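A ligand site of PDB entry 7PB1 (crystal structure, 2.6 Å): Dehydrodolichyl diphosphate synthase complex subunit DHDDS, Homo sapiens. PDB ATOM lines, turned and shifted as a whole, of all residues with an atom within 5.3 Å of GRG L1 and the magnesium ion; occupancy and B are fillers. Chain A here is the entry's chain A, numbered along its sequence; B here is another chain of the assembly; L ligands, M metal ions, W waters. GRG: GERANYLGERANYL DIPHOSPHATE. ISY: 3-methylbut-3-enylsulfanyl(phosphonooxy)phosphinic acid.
The magnesium ion is bound by an oxygen (O3B) of GRG L1 (1.9 Å), water W1 (2.0 Å), the side-chain carboxylate (OD1) of Asp 41 (2.2 Å), an oxygen (O7) of ISY L2 (2.2 Å), an oxygen (O2A) of GRG L1 (2.2 Å) and water W2 (2.2 Å).
Water W1 bridges NE of Arg 216 of chain B and O2B of GRG L1.
The backbone NH (N) of Arg 45 lies within hydrogen-bond range of an oxygen (O1B) of GRG L1 (2.8 Å).
O1B of GRG L1 is in salt-bridge range of NE of Arg 45 (2.7 Å).
An oxygen (O1A) of GRG L1 lies within salt-bridge range of the guanidinium group (NH1) of Arg 92 (2.9 Å).
The backbone NH of Arg 44 sits at hydrogen-bond distance from an oxygen (O3A) of GRG L1, 2.9 Å away.
NH1 of Arg 44 is in salt-bridge range of O2B of GRG L1.
N of Asn 43 lies within hydrogen-bond range of O3A of GRG L1 (2.9 Å).
An oxygen (O1A) of GRG L1 lies close to a ring nitrogen (NE2) of His 58 (3.5 Å).
N of Gly 42 sits close to O3A of GRG L1.
The guanidinium group (NH2) of Arg 92 is in salt-bridge range of an oxygen (O8) of ISY L2 (3.7 Å).
An oxygen (O8) of ISY L2 sits at hydrogen-bond distance from the side-chain amide nitrogen (ND2) of Asn 89 (3.4 Å).
NE of Arg 216 of chain B lies within salt-bridge range of O5 of ISY L2, 3.7 Å away.
NH2 of Arg 212 is in salt-bridge range of O5 of ISY L2.
The guanidinium group (NH2) of Arg 45 is in salt-bridge range of the side-chain carboxylate (OD2) of Asp 41, 3.4 Å away.
The guanidinium group (NH2) of Arg 212 lies within salt-bridge range of the side-chain carboxylate (OD2) of Asp 41 (2.8 Å).
The side-chain hydroxyl (OG) of Ser 214 is in hydrogen-bond range of the side-chain carboxylate (OD2) of Asp 41 (3.3 Å).
The guanidinium group of Arg 45 lies within hydrogen-bond range of the side-chain hydroxyl of Ser 214 (3.1 Å).
NH2 of Arg 92 lies close to ND2 of Asn 89, 3.0 Å away.
ND1 of His 58 lies within hydrogen-bond range of ND2 of Asn 43, 3.0 Å away.
Met 40 touches GRG L1 (O to C2, 2.9 Å).
CE1 of Phe 62 touches C16 of GRG L1, at 3.4 Å.
Leu 65 touches GRG L1 (CD2 to C11, 3.6 Å).
Ala 84 touches GRG L1 (O to C5, 3.0 Å).
Asn 89 touches GRG L1 (OD1 to C4, 3.96 Å).
Leu 103 touches GRG L1 (CD2 to C10, 3.6 Å).
Ala 104 touches GRG L1 (CA to C14, 3.5 Å).
Phe 108 touches GRG L1 (CZ to C17, 3.8 Å).
Leu 111 touches GRG L1 (CD1 to C19, 3.8 Å).
Ile 125 touches GRG L1.
Val 159 touches GRG L1.
CE2 of Phe 161 touches C14 of GRG L1, at 3.9 Å.
Hydrophobic or aromatic side chains within 4 Å of GRG L1: Met 40, His 58, Phe 62, Leu 65, Leu 103, Ala 104, Phe 108, Leu 111, Ile 125, Val 159 and Phe 161.
19 residues have an atom within 4 Å of GRG L1: Met 40, Asp 41, Gly 42, Asn 43, Arg 44, Arg 45, His 58, Phe 62, Leu 65, Ala 84, Asn 89, Arg 92, Leu 103, Ala 104, Phe 108, Leu 111, Ile 125, Val 159 and Phe 161.
NH2 of Arg 45 touches the magnesium ion, 3.6 Å away.
Of the 29 residues printed, 2 come within 4 Å of the magnesium ion.
The nearest printed residue that does not touch the magnesium ion is Gly 42 (4.1 Å).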
ATOM      1  N   MET A  40       9.349  -4.550  14.749  1.00  0.00           N
ATOM      2  CA  MET A  40       9.121  -5.711  13.908  1.00  0.00           C
ATOM      3  C   MET A  40       7.755  -6.317  14.215  1.00  0.00           C
ATOM      4  O   MET A  40       7.624  -7.205  15.054  1.00  0.00           O
ATOM      5  CB  MET A  40      10.229  -6.744  14.126  1.00  0.00           C
ATOM      6  CG  MET A  40      11.613  -6.112  14.196  1.00  0.00           C
ATOM      7  SD  MET A  40      12.964  -7.284  14.479  1.00  0.00           S
ATOM      8  CE  MET A  40      12.630  -7.804  16.154  1.00  0.00           C
ATOM      9  N   ASP A  41       6.730  -5.827  13.528  1.00  0.00           N
ATOM     10  CA  ASP A  41       5.346  -6.186  13.820  1.00  0.00           C
ATOM     11  C   ASP A  41       4.736  -6.939  12.645  1.00  0.00           C
ATOM     12  O   ASP A  41       5.124  -6.722  11.490  1.00  0.00           O
ATOM     13  CB  ASP A  41       4.534  -4.919  14.128  1.00  0.00           C
ATOM     14  CG  ASP A  41       3.303  -5.207  14.942  1.00  0.00           C
ATOM     15  OD1 ASP A  41       3.301  -6.250  15.632  1.00  0.00           O
ATOM     16  OD2 ASP A  41       2.354  -4.395  14.899  1.00  0.00           O
ATOM     17  N   GLY A  42       3.801  -7.835  12.943  1.00  0.00           N
ATOM     18  CA  GLY A  42       3.107  -8.598  11.928  1.00  0.00           C
ATOM     19  C   GLY A  42       3.511 -10.060  11.798  1.00  0.00           C
ATOM     20  O   GLY A  42       3.029 -10.732  10.883  1.00  0.00           O
ATOM     21  N   ASN A  43       4.355 -10.574  12.698  1.00  0.00           N
ATOM     22  CA  ASN A  43       4.844 -11.945  12.570  1.00  0.00           C
ATOM     23  C   ASN A  43       3.714 -12.957  12.577  1.00  0.00           C
ATOM     24  O   ASN A  43       3.719 -13.915  11.783  1.00  0.00           O
ATOM     25  CB  ASN A  43       5.821 -12.250  13.703  1.00  0.00           C
ATOM     26  CG  ASN A  43       7.200 -11.678  13.450  1.00  0.00           C
ATOM     27  OD1 ASN A  43       7.391 -10.840  12.556  1.00  0.00           O
ATOM     28  ND2 ASN A  43       8.177 -12.125  14.233  1.00  0.00           N
ATOM     29  N   ARG A  44       2.720 -12.780  13.454  1.00  0.00           N
ATOM     30  CA  ARG A  44       1.644 -13.766  13.553  1.00  0.00           C
ATOM     31  C   ARG A  44       0.704 -13.687  12.354  1.00  0.00           C
ATOM     32  O   ARG A  44       0.247 -14.724  11.849  1.00  0.00           O
ATOM     33  CB  ARG A  44       0.875 -13.574  14.846  1.00  0.00           C
ATOM     34  CG  ARG A  44       1.641 -14.001  16.083  1.00  0.00           C
ATOM     35  CD  ARG A  44       1.352 -13.056  17.217  1.00  0.00           C
ATOM     36  NE  ARG A  44       0.162 -13.418  17.977  1.00  0.00           N
ATOM     37  CZ  ARG A  44      -0.453 -12.613  18.822  1.00  0.00           C
ATOM     38  NH1 ARG A  44       0.002 -11.383  19.009  1.00  0.00           N
ATOM     39  NH2 ARG A  44      -1.532 -13.019  19.473  1.00  0.00           N
ATOM     40  N   ARG A  45       0.386 -12.474  11.906  1.00  0.00           N
ATOM     41  CA  ARG A  45      -0.489 -12.338  10.747  1.00  0.00           C
ATOM     42  C   ARG A  45       0.147 -12.984   9.520  1.00  0.00           C
ATOM     43  O   ARG A  45      -0.535 -13.671   8.741  1.00  0.00           O
ATOM     44  CB  ARG A  45      -0.788 -10.866  10.481  1.00  0.00           C
ATOM     45  CG  ARG A  45      -1.913 -10.302  11.321  1.00  0.00           C
ATOM     46  CD  ARG A  45      -1.875  -8.795  11.300  1.00  0.00           C
ATOM     47  NE  ARG A  45      -0.901  -8.243  12.236  1.00  0.00           N
ATOM     48  CZ  ARG A  45      -0.612  -6.949  12.313  1.00  0.00           C
ATOM     49  NH1 ARG A  45      -1.215  -6.081  11.509  1.00  0.00           N
ATOM     50  NH2 ARG A  45       0.284  -6.515  13.195  1.00  0.00           N
ATOM     51  N   TYR A  46       1.448 -12.772   9.342  1.00  0.00           N
ATOM     52  CA  TYR A  46       2.190 -13.446   8.283  1.00  0.00           C
ATOM     53  C   TYR A  46       2.025 -14.951   8.385  1.00  0.00           C
ATOM     54  O   TYR A  46       1.711 -15.612   7.386  1.00  0.00           O
ATOM     55  CB  TYR A  46       3.657 -13.049   8.345  1.00  0.00           C
ATOM     56  CG  TYR A  46       4.584 -13.936   7.551  1.00  0.00           C
ATOM     57  CD1 TYR A  46       4.802 -13.704   6.197  1.00  0.00           C
ATOM     58  CD2 TYR A  46       5.248 -15.002   8.164  1.00  0.00           C
ATOM     59  CE1 TYR A  46       5.662 -14.526   5.466  1.00  0.00           C
ATOM     60  CE2 TYR A  46       6.096 -15.817   7.437  1.00  0.00           C
ATOM     61  CZ  TYR A  46       6.302 -15.580   6.088  1.00  0.00           C
ATOM     62  OH  TYR A  46       7.141 -16.394   5.379  1.00  0.00           O
ATOM     63  N   HIS A  58       7.465 -16.370  13.837  1.00  0.00           N
ATOM     64  CA  HIS A  58       8.471 -15.667  14.632  1.00  0.00           C
ATOM     65  C   HIS A  58       9.881 -16.086  14.262  1.00  0.00           C
ATOM     66  O   HIS A  58      10.815 -15.279  14.363  1.00  0.00           O
ATOM     67  CB  HIS A  58       8.218 -15.921  16.116  1.00  0.00           C
ATOM     68  CG  HIS A  58       7.099 -15.120  16.684  1.00  0.00           C
ATOM     69  ND1 HIS A  58       6.991 -13.752  16.477  1.00  0.00           N
ATOM     70  CD2 HIS A  58       6.044 -15.463  17.455  1.00  0.00           C
ATOM     71  CE1 HIS A  58       5.913 -13.306  17.091  1.00  0.00           C
ATOM     72  NE2 HIS A  58       5.323 -14.323  17.695  1.00  0.00           N
ATOM     73  N   GLY A  61      10.356 -14.317  11.223  1.00  0.00           N
ATOM     74  CA  GLY A  61      10.569 -12.942  11.649  1.00  0.00           C
ATOM     75  C   GLY A  61      11.992 -12.673  12.079  1.00  0.00           C
ATOM     76  O   GLY A  61      12.536 -11.589  11.851  1.00  0.00           O
ATOM     77  N   PHE A  62      12.633 -13.677  12.698  1.00  0.00           N
ATOM     78  CA  PHE A  62      14.018 -13.474  13.103  1.00  0.00           C
ATOM     79  C   PHE A  62      14.954 -13.471  11.914  1.00  0.00           C
ATOM     80  O   PHE A  62      15.869 -12.633  11.845  1.00  0.00           O
ATOM     81  CB  PHE A  62      14.441 -14.556  14.100  1.00  0.00           C
ATOM     82  CG  PHE A  62      15.901 -14.505  14.430  1.00  0.00           C
ATOM     83  CD1 PHE A  62      16.385 -13.607  15.362  1.00  0.00           C
ATOM     84  CD2 PHE A  62      16.797 -15.333  13.773  1.00  0.00           C
ATOM     85  CE1 PHE A  62      17.725 -13.542  15.653  1.00  0.00           C
ATOM     86  CE2 PHE A  62      18.149 -15.274  14.059  1.00  0.00           C
ATOM     87  CZ  PHE A  62      18.607 -14.377  15.012  1.00  0.00           C
ATOM     88  N   LEU A  65      15.046  -9.977  10.534  1.00  0.00           N
ATOM     89  CA  LEU A  65      15.893  -9.100  11.338  1.00  0.00           C
ATOM     90  C   LEU A  65      17.368  -9.285  10.985  1.00  0.00           C
ATOM     91  O   LEU A  65      18.128  -8.309  10.963  1.00  0.00           O
ATOM     92  CB  LEU A  65      15.672  -9.378  12.829  1.00  0.00           C
ATOM     93  CG  LEU A  65      16.793  -8.921  13.767  1.00  0.00           C
ATOM     94  CD1 LEU A  65      16.833  -7.411  13.871  1.00  0.00           C
ATOM     95  CD2 LEU A  65      16.649  -9.536  15.141  1.00  0.00           C
ATOM     96  N   TYR A  83      12.681  -3.626  18.377  1.00  0.00           N
ATOM     97  CA  TYR A  83      11.735  -4.002  19.430  1.00  0.00           C
ATOM     98  C   TYR A  83      11.492  -5.498  19.311  1.00  0.00           C
ATOM     99  O   TYR A  83      10.761  -5.953  18.425  1.00  0.00           O
ATOM    100  CB  TYR A  83      10.451  -3.200  19.274  1.00  0.00           C
ATOM    101  CG  TYR A  83       9.681  -2.968  20.553  1.00  0.00           C
ATOM    102  CD1 TYR A  83       8.622  -2.067  20.583  1.00  0.00           C
ATOM    103  CD2 TYR A  83       9.983  -3.660  21.719  1.00  0.00           C
ATOM    104  CE1 TYR A  83       7.903  -1.846  21.731  1.00  0.00           C
ATOM    105  CE2 TYR A  83       9.253  -3.447  22.874  1.00  0.00           C
ATOM    106  CZ  TYR A  83       8.218  -2.540  22.870  1.00  0.00           C
ATOM    107  OH  TYR A  83       7.478  -2.293  24.017  1.00  0.00           O
ATOM    108  N   ALA A  84      12.105  -6.273  20.203  1.00  0.00           N
ATOM    109  CA  ALA A  84      12.085  -7.727  20.117  1.00  0.00           C
ATOM    110  C   ALA A  84      11.073  -8.381  21.043  1.00  0.00           C
ATOM    111  O   ALA A  84      10.545  -9.440  20.706  1.00  0.00           O
ATOM    112  CB  ALA A  84      13.474  -8.294  20.420  1.00  0.00           C
ATOM    113  N   PHE A  85      10.811  -7.794  22.217  1.00  0.00           N
ATOM    114  CA  PHE A  85       9.821  -8.370  23.116  1.00  0.00           C
ATOM    115  C   PHE A  85       9.384  -7.305  24.111  1.00  0.00           C
ATOM    116  O   PHE A  85      10.209  -6.809  24.885  1.00  0.00           O
ATOM    117  CB  PHE A  85      10.381  -9.584  23.855  1.00  0.00           C
ATOM    118  CG  PHE A  85       9.318 -10.445  24.479  1.00  0.00           C
ATOM    119  CD1 PHE A  85       8.955 -10.259  25.809  1.00  0.00           C
ATOM    120  CD2 PHE A  85       8.668 -11.417  23.736  1.00  0.00           C
ATOM    121  CE1 PHE A  85       7.965 -11.045  26.386  1.00  0.00           C
ATOM    122  CE2 PHE A  85       7.687 -12.195  24.306  1.00  0.00           C
ATOM    123  CZ  PHE A  85       7.336 -12.016  25.632  1.00  0.00           C
ATOM    124  N   ASN A  89       3.840  -8.088  25.991  1.00  0.00           N
ATOM    125  CA  ASN A  89       3.751  -9.413  25.389  1.00  0.00           C
ATOM    126  C   ASN A  89       3.784 -10.542  26.417  1.00  0.00           C
ATOM    127  O   ASN A  89       3.481 -11.682  26.063  1.00  0.00           O
ATOM    128  CB  ASN A  89       4.878  -9.605  24.377  1.00  0.00           C
ATOM    129  CG  ASN A  89       4.832  -8.591  23.261  1.00  0.00           C
ATOM    130  OD1 ASN A  89       5.866  -8.049  22.858  1.00  0.00           O
ATOM    131  ND2 ASN A  89       3.641  -8.339  22.731  1.00  0.00           N
ATOM    132  N   ARG A  92       0.575 -12.784  26.594  1.00  0.00           N
ATOM    133  CA  ARG A  92       0.174 -13.739  25.583  1.00  0.00           C
ATOM    134  C   ARG A  92       0.086 -15.135  26.198  1.00  0.00           C
ATOM    135  O   ARG A  92       0.337 -15.326  27.394  1.00  0.00           O
ATOM    136  CB  ARG A  92       1.142 -13.709  24.397  1.00  0.00           C
ATOM    137  CG  ARG A  92       1.270 -12.325  23.769  1.00  0.00           C
ATOM    138  CD  ARG A  92       1.919 -12.333  22.402  1.00  0.00           C
ATOM    139  NE  ARG A  92       1.937 -11.000  21.823  1.00  0.00           N
ATOM    140  CZ  ARG A  92       2.437 -10.687  20.628  1.00  0.00           C
ATOM    141  NH1 ARG A  92       2.986 -11.627  19.860  1.00  0.00           N
ATOM    142  NH2 ARG A  92       2.406  -9.433  20.198  1.00  0.00           N
ATOM    143  N   LEU A 100       8.575 -17.823  22.257  1.00  0.00           N
ATOM    144  CA  LEU A 100       9.459 -16.675  22.061  1.00  0.00           C
ATOM    145  C   LEU A 100      10.712 -16.795  22.915  1.00  0.00           C
ATOM    146  O   LEU A 100      11.828 -16.511  22.449  1.00  0.00           O
ATOM    147  CB  LEU A 100       8.739 -15.373  22.380  1.00  0.00           C
ATOM    148  CG  LEU A 100       7.863 -14.722  21.307  1.00  0.00           C
ATOM    149  CD1 LEU A 100       8.598 -14.672  19.969  1.00  0.00           C
ATOM    150  CD2 LEU A 100       6.512 -15.422  21.180  1.00  0.00           C
ATOM    151  N   LEU A 103      13.117 -19.224  21.529  1.00  0.00           N
ATOM    152  CA  LEU A 103      13.744 -18.664  20.336  1.00  0.00           C
ATOM    153  C   LEU A 103      14.880 -17.720  20.719  1.00  0.00           C
ATOM    154  O   LEU A 103      15.958 -17.749  20.099  1.00  0.00           O
ATOM    155  CB  LEU A 103      12.701 -17.948  19.478  1.00  0.00           C
ATOM    156  CG  LEU A 103      13.220 -17.438  18.132  1.00  0.00           C
ATOM    157  CD1 LEU A 103      13.343 -18.580  17.141  1.00  0.00           C
ATOM    158  CD2 LEU A 103      12.302 -16.360  17.592  1.00  0.00           C
ATOM    159  N   ALA A 104      14.673 -16.914  21.759  1.00  0.00           N
ATOM    160  CA  ALA A 104      15.743 -16.019  22.214  1.00  0.00           C
ATOM    161  C   ALA A 104      16.891 -16.808  22.804  1.00  0.00           C
ATOM    162  O   ALA A 104      18.066 -16.467  22.588  1.00  0.00           O
ATOM    163  CB  ALA A 104      15.192 -15.017  23.223  1.00  0.00           C
ATOM    164  N   LYS A 107      18.801 -18.255  19.763  1.00  0.00           N
ATOM    165  CA  LYS A 107      19.595 -17.314  18.986  1.00  0.00           C
ATOM    166  C   LYS A 107      20.740 -16.720  19.803  1.00  0.00           C
ATOM    167  O   LYS A 107      21.873 -16.623  19.313  1.00  0.00           O
ATOM    168  CB  LYS A 107      18.693 -16.215  18.419  1.00  0.00           C
ATOM    169  CG  LYS A 107      17.748 -16.753  17.351  1.00  0.00           C
ATOM    170  CD  LYS A 107      18.467 -17.778  16.484  1.00  0.00           C
ATOM    171  CE  LYS A 107      17.579 -18.375  15.405  1.00  0.00           C
ATOM    172  NZ  LYS A 107      18.393 -19.229  14.484  1.00  0.00           N
ATOM    173  N   PHE A 108      20.477 -16.323  21.056  1.00  0.00           N
ATOM    174  CA  PHE A 108      21.558 -15.832  21.915  1.00  0.00           C
ATOM    175  C   PHE A 108      22.617 -16.894  22.178  1.00  0.00           C
ATOM    176  O   PHE A 108      23.752 -16.547  22.513  1.00  0.00           O
ATOM    177  CB  PHE A 108      21.010 -15.304  23.240  1.00  0.00           C
ATOM    178  CG  PHE A 108      20.567 -13.866  23.184  1.00  0.00           C
ATOM    179  CD1 PHE A 108      21.494 -12.841  23.210  1.00  0.00           C
ATOM    180  CD2 PHE A 108      19.211 -13.547  23.094  1.00  0.00           C
ATOM    181  CE1 PHE A 108      21.086 -11.521  23.146  1.00  0.00           C
ATOM    182  CE2 PHE A 108      18.806 -12.232  23.043  1.00  0.00           C
ATOM    183  CZ  PHE A 108      19.744 -11.213  23.064  1.00  0.00           C
ATOM    184  N   LEU A 111      24.865 -17.094  19.084  1.00  0.00           N
ATOM    185  CA  LEU A 111      25.718 -15.911  19.016  1.00  0.00           C
ATOM    186  C   LEU A 111      27.079 -16.186  19.633  1.00  0.00           C
ATOM    187  O   LEU A 111      28.096 -15.673  19.145  1.00  0.00           O
ATOM    188  CB  LEU A 111      25.045 -14.738  19.715  1.00  0.00           C
ATOM    189  CG  LEU A 111      23.926 -14.064  18.934  1.00  0.00           C
ATOM    190  CD1 LEU A 111      23.855 -12.608  19.334  1.00  0.00           C
ATOM    191  CD2 LEU A 111      24.169 -14.216  17.440  1.00  0.00           C
ATOM    192  N   ILE A 125      26.602  -5.698  20.727  1.00  0.00           N
ATOM    193  CA  ILE A 125      25.231  -6.126  21.019  1.00  0.00           C
ATOM    194  C   ILE A 125      24.842  -5.579  22.389  1.00  0.00           C
ATOM    195  O   ILE A 125      25.497  -5.873  23.391  1.00  0.00           O
ATOM    196  CB  ILE A 125      25.082  -7.647  20.995  1.00  0.00           C
ATOM    197  CG1 ILE A 125      25.473  -8.235  19.640  1.00  0.00           C
ATOM    198  CG2 ILE A 125      23.645  -8.034  21.341  1.00  0.00           C
ATOM    199  CD1 ILE A 125      24.299  -8.475  18.705  1.00  0.00           C
ATOM    200  N   LEU A 157      23.981  -3.075  17.500  1.00  0.00           N
ATOM    201  CA  LEU A 157      22.598  -3.544  17.509  1.00  0.00           C
ATOM    202  C   LEU A 157      22.042  -3.410  18.913  1.00  0.00           C
ATOM    203  O   LEU A 157      22.694  -3.840  19.879  1.00  0.00           O
ATOM    204  CB  LEU A 157      22.482  -4.980  17.024  1.00  0.00           C
ATOM    205  CG  LEU A 157      21.035  -5.470  16.945  1.00  0.00           C
ATOM    206  CD1 LEU A 157      20.271  -4.678  15.897  1.00  0.00           C
ATOM    207  CD2 LEU A 157      20.957  -6.967  16.652  1.00  0.00           C
ATOM    208  N   VAL A 159      18.748  -4.454  21.140  1.00  0.00           N
ATOM    209  CA  VAL A 159      17.635  -5.391  21.149  1.00  0.00           C
ATOM    210  C   VAL A 159      16.827  -5.117  22.405  1.00  0.00           C
ATOM    211  O   VAL A 159      17.293  -5.332  23.532  1.00  0.00           O
ATOM    212  CB  VAL A 159      18.117  -6.853  21.103  1.00  0.00           C
ATOM    213  CG1 VAL A 159      16.914  -7.794  21.067  1.00  0.00           C
ATOM    214  CG2 VAL A 159      19.012  -7.060  19.886  1.00  0.00           C
ATOM    215  N   PHE A 161      14.376  -6.078  24.839  1.00  0.00           N
ATOM    216  CA  PHE A 161      13.773  -7.314  25.329  1.00  0.00           C
ATOM    217  C   PHE A 161      13.163  -7.062  26.698  1.00  0.00           C
ATOM    218  O   PHE A 161      13.874  -6.708  27.649  1.00  0.00           O
ATOM    219  CB  PHE A 161      14.802  -8.451  25.390  1.00  0.00           C
ATOM    220  CG  PHE A 161      14.282  -9.749  24.826  1.00  0.00           C
ATOM    221  CD1 PHE A 161      13.657 -10.685  25.632  1.00  0.00           C
ATOM    222  CD2 PHE A 161      14.420 -10.025  23.467  1.00  0.00           C
ATOM    223  CE1 PHE A 161      13.164 -11.874  25.097  1.00  0.00           C
ATOM    224  CE2 PHE A 161      13.935 -11.220  22.937  1.00  0.00           C
ATOM    225  CZ  PHE A 161      13.311 -12.148  23.753  1.00  0.00           C
ATOM    226  N   ARG A 212       7.653   1.084  11.856  1.00  0.00           N
ATOM    227  CA  ARG A 212       6.714   0.064  12.307  1.00  0.00           C
ATOM    228  C   ARG A 212       6.058  -0.577  11.100  1.00  0.00           C
ATOM    229  O   ARG A 212       5.554   0.127  10.212  1.00  0.00           O
ATOM    230  CB  ARG A 212       5.636   0.611  13.239  1.00  0.00           C
ATOM    231  CG  ARG A 212       4.588  -0.453  13.571  1.00  0.00           C
ATOM    232  CD  ARG A 212       3.936  -0.222  14.887  1.00  0.00           C
ATOM    233  NE  ARG A 212       3.313  -1.418  15.420  1.00  0.00           N
ATOM    234  CZ  ARG A 212       2.680  -1.456  16.595  1.00  0.00           C
ATOM    235  NH1 ARG A 212       2.597  -0.358  17.329  1.00  0.00           N
ATOM    236  NH2 ARG A 212       2.139  -2.583  17.031  1.00  0.00           N
ATOM    237  N   SER A 214       3.452  -3.761   9.291  1.00  0.00           N
ATOM    238  CA  SER A 214       2.014  -4.022   9.246  1.00  0.00           C
ATOM    239  C   SER A 214       1.264  -2.703   9.245  1.00  0.00           C
ATOM    240  O   SER A 214       1.863  -1.626   9.280  1.00  0.00           O
ATOM    241  CB  SER A 214       1.573  -4.914  10.410  1.00  0.00           C
ATOM    242  OG  SER A 214       1.618  -4.226  11.653  1.00  0.00           O
ATOM    243  N   ARG B 216      -4.526  -4.149  19.848  1.00  0.00           N
ATOM    244  CA  ARG B 216      -4.318  -5.455  20.461  1.00  0.00           C
ATOM    245  C   ARG B 216      -3.709  -5.365  21.840  1.00  0.00           C
ATOM    246  O   ARG B 216      -3.853  -6.305  22.630  1.00  0.00           O
ATOM    247  CB  ARG B 216      -3.436  -6.320  19.553  1.00  0.00           C
ATOM    248  CG  ARG B 216      -4.216  -7.092  18.506  1.00  0.00           C
ATOM    249  CD  ARG B 216      -3.293  -7.804  17.519  1.00  0.00           C
ATOM    250  NE  ARG B 216      -2.508  -6.875  16.716  1.00  0.00           N
ATOM    251  CZ  ARG B 216      -2.998  -6.172  15.700  1.00  0.00           C
ATOM    252  NH1 ARG B 216      -4.282  -6.288  15.363  1.00  0.00           N
ATOM    253  NH2 ARG B 216      -2.203  -5.346  15.033  1.00  0.00           N
HETATM  254  C20 GRG L   1      20.163 -11.256  17.160  1.00  0.00           C
HETATM  255  C19 GRG L   1      21.112 -10.013  19.269  1.00  0.00           C
HETATM  256  C18 GRG L   1      19.999 -10.827  18.608  1.00  0.00           C
HETATM  257  C17 GRG L   1      18.915 -11.138  19.328  1.00  0.00           C
HETATM  258  C16 GRG L   1      17.757 -11.958  18.711  1.00  0.00           C
HETATM  259  C14 GRG L   1      15.399 -13.344  19.953  1.00  0.00           C
HETATM  260  C13 GRG L   1      15.291 -12.217  18.933  1.00  0.00           C
HETATM  261  C15 GRG L   1      16.429 -11.179  18.850  1.00  0.00           C
HETATM  262  C12 GRG L   1      14.213 -12.184  18.116  1.00  0.00           C
HETATM  263  C11 GRG L   1      14.009 -11.078  17.037  1.00  0.00           C
HETATM  264  C9  GRG L   1      12.979 -11.557  15.956  1.00  0.00           C
HETATM  265  C8  GRG L   1      11.547 -11.730  16.547  1.00  0.00           C
HETATM  266  C10 GRG L   1      11.103 -13.037  17.201  1.00  0.00           C
HETATM  267  C7  GRG L   1      10.652 -10.741  16.485  1.00  0.00           C
HETATM  268  C6  GRG L   1       9.256 -10.992  17.100  1.00  0.00           C
HETATM  269  C5  GRG L   1       8.958  -9.968  18.236  1.00  0.00           C
HETATM  270  C3  GRG L   1       7.461  -9.663  18.277  1.00  0.00           C
HETATM  271  C4  GRG L   1       6.622 -10.008  19.506  1.00  0.00           C
HETATM  272  C2  GRG L   1       6.920  -9.101  17.178  1.00  0.00           C
HETATM  273  C1  GRG L   1       5.446  -8.722  17.059  1.00  0.00           C
HETATM  274  O1  GRG L   1       4.854  -9.301  15.925  1.00  0.00           O
HETATM  275  PA  GRG L   1       3.411 -10.018  16.336  1.00  0.00           P
HETATM  276  O1A GRG L   1       3.721 -11.284  17.098  1.00  0.00           O
HETATM  277  O3A GRG L   1       2.539 -10.321  14.974  1.00  0.00           O
HETATM  278  O2A GRG L   1       2.603  -9.129  17.245  1.00  0.00           O
HETATM  279  PB  GRG L   1       1.022  -9.735  14.828  1.00  0.00           P
HETATM  280  O1B GRG L   1       0.444 -10.179  13.512  1.00  0.00           O
HETATM  281  O2B GRG L   1       0.209 -10.251  15.992  1.00  0.00           O
HETATM  282  O3B GRG L   1       1.068  -8.235  14.858  1.00  0.00           O
HETATM  283  P1  ISY L   2       0.095  -4.000  19.634  1.00  0.00           P
HETATM  284  O2  ISY L   2       1.554  -4.184  18.937  1.00  0.00           O
HETATM  285  P3  ISY L   2       2.492  -5.486  19.300  1.00  0.00           P
HETATM  286  O4  ISY L   2       0.027  -2.678  20.360  1.00  0.00           O
HETATM  287  O5  ISY L   2      -0.960  -4.085  18.558  1.00  0.00           O
HETATM  288  O6  ISY L   2      -0.082  -5.167  20.582  1.00  0.00           O
HETATM  289  O7  ISY L   2       2.095  -6.669  18.454  1.00  0.00           O
HETATM  290  O8  ISY L   2       2.375  -5.825  20.769  1.00  0.00           O
HETATM  291  S9  ISY L   2       4.468  -4.898  18.898  1.00  0.00           S
HETATM  292  C10 ISY L   2       5.287  -5.169  20.487  1.00  0.00           C
HETATM  293  C11 ISY L   2       6.768  -4.827  20.347  1.00  0.00           C
HETATM  294  C12 ISY L   2       7.452  -5.938  19.569  1.00  0.00           C
HETATM  295  C13 ISY L   2       7.627  -5.821  18.056  1.00  0.00           C
HETATM  296  C14 ISY L   2       7.879  -6.994  20.219  1.00  0.00           C
HETATM  297 MG    MG M   1       1.651  -7.355  16.459  1.00  0.00          MG
HETATM  298  O   HOH W   1      -0.141  -7.803  17.225  1.00  0.00           O
HETATM  299  O   HOH W   2       0.537  -5.484  16.370  1.00  0.00           O
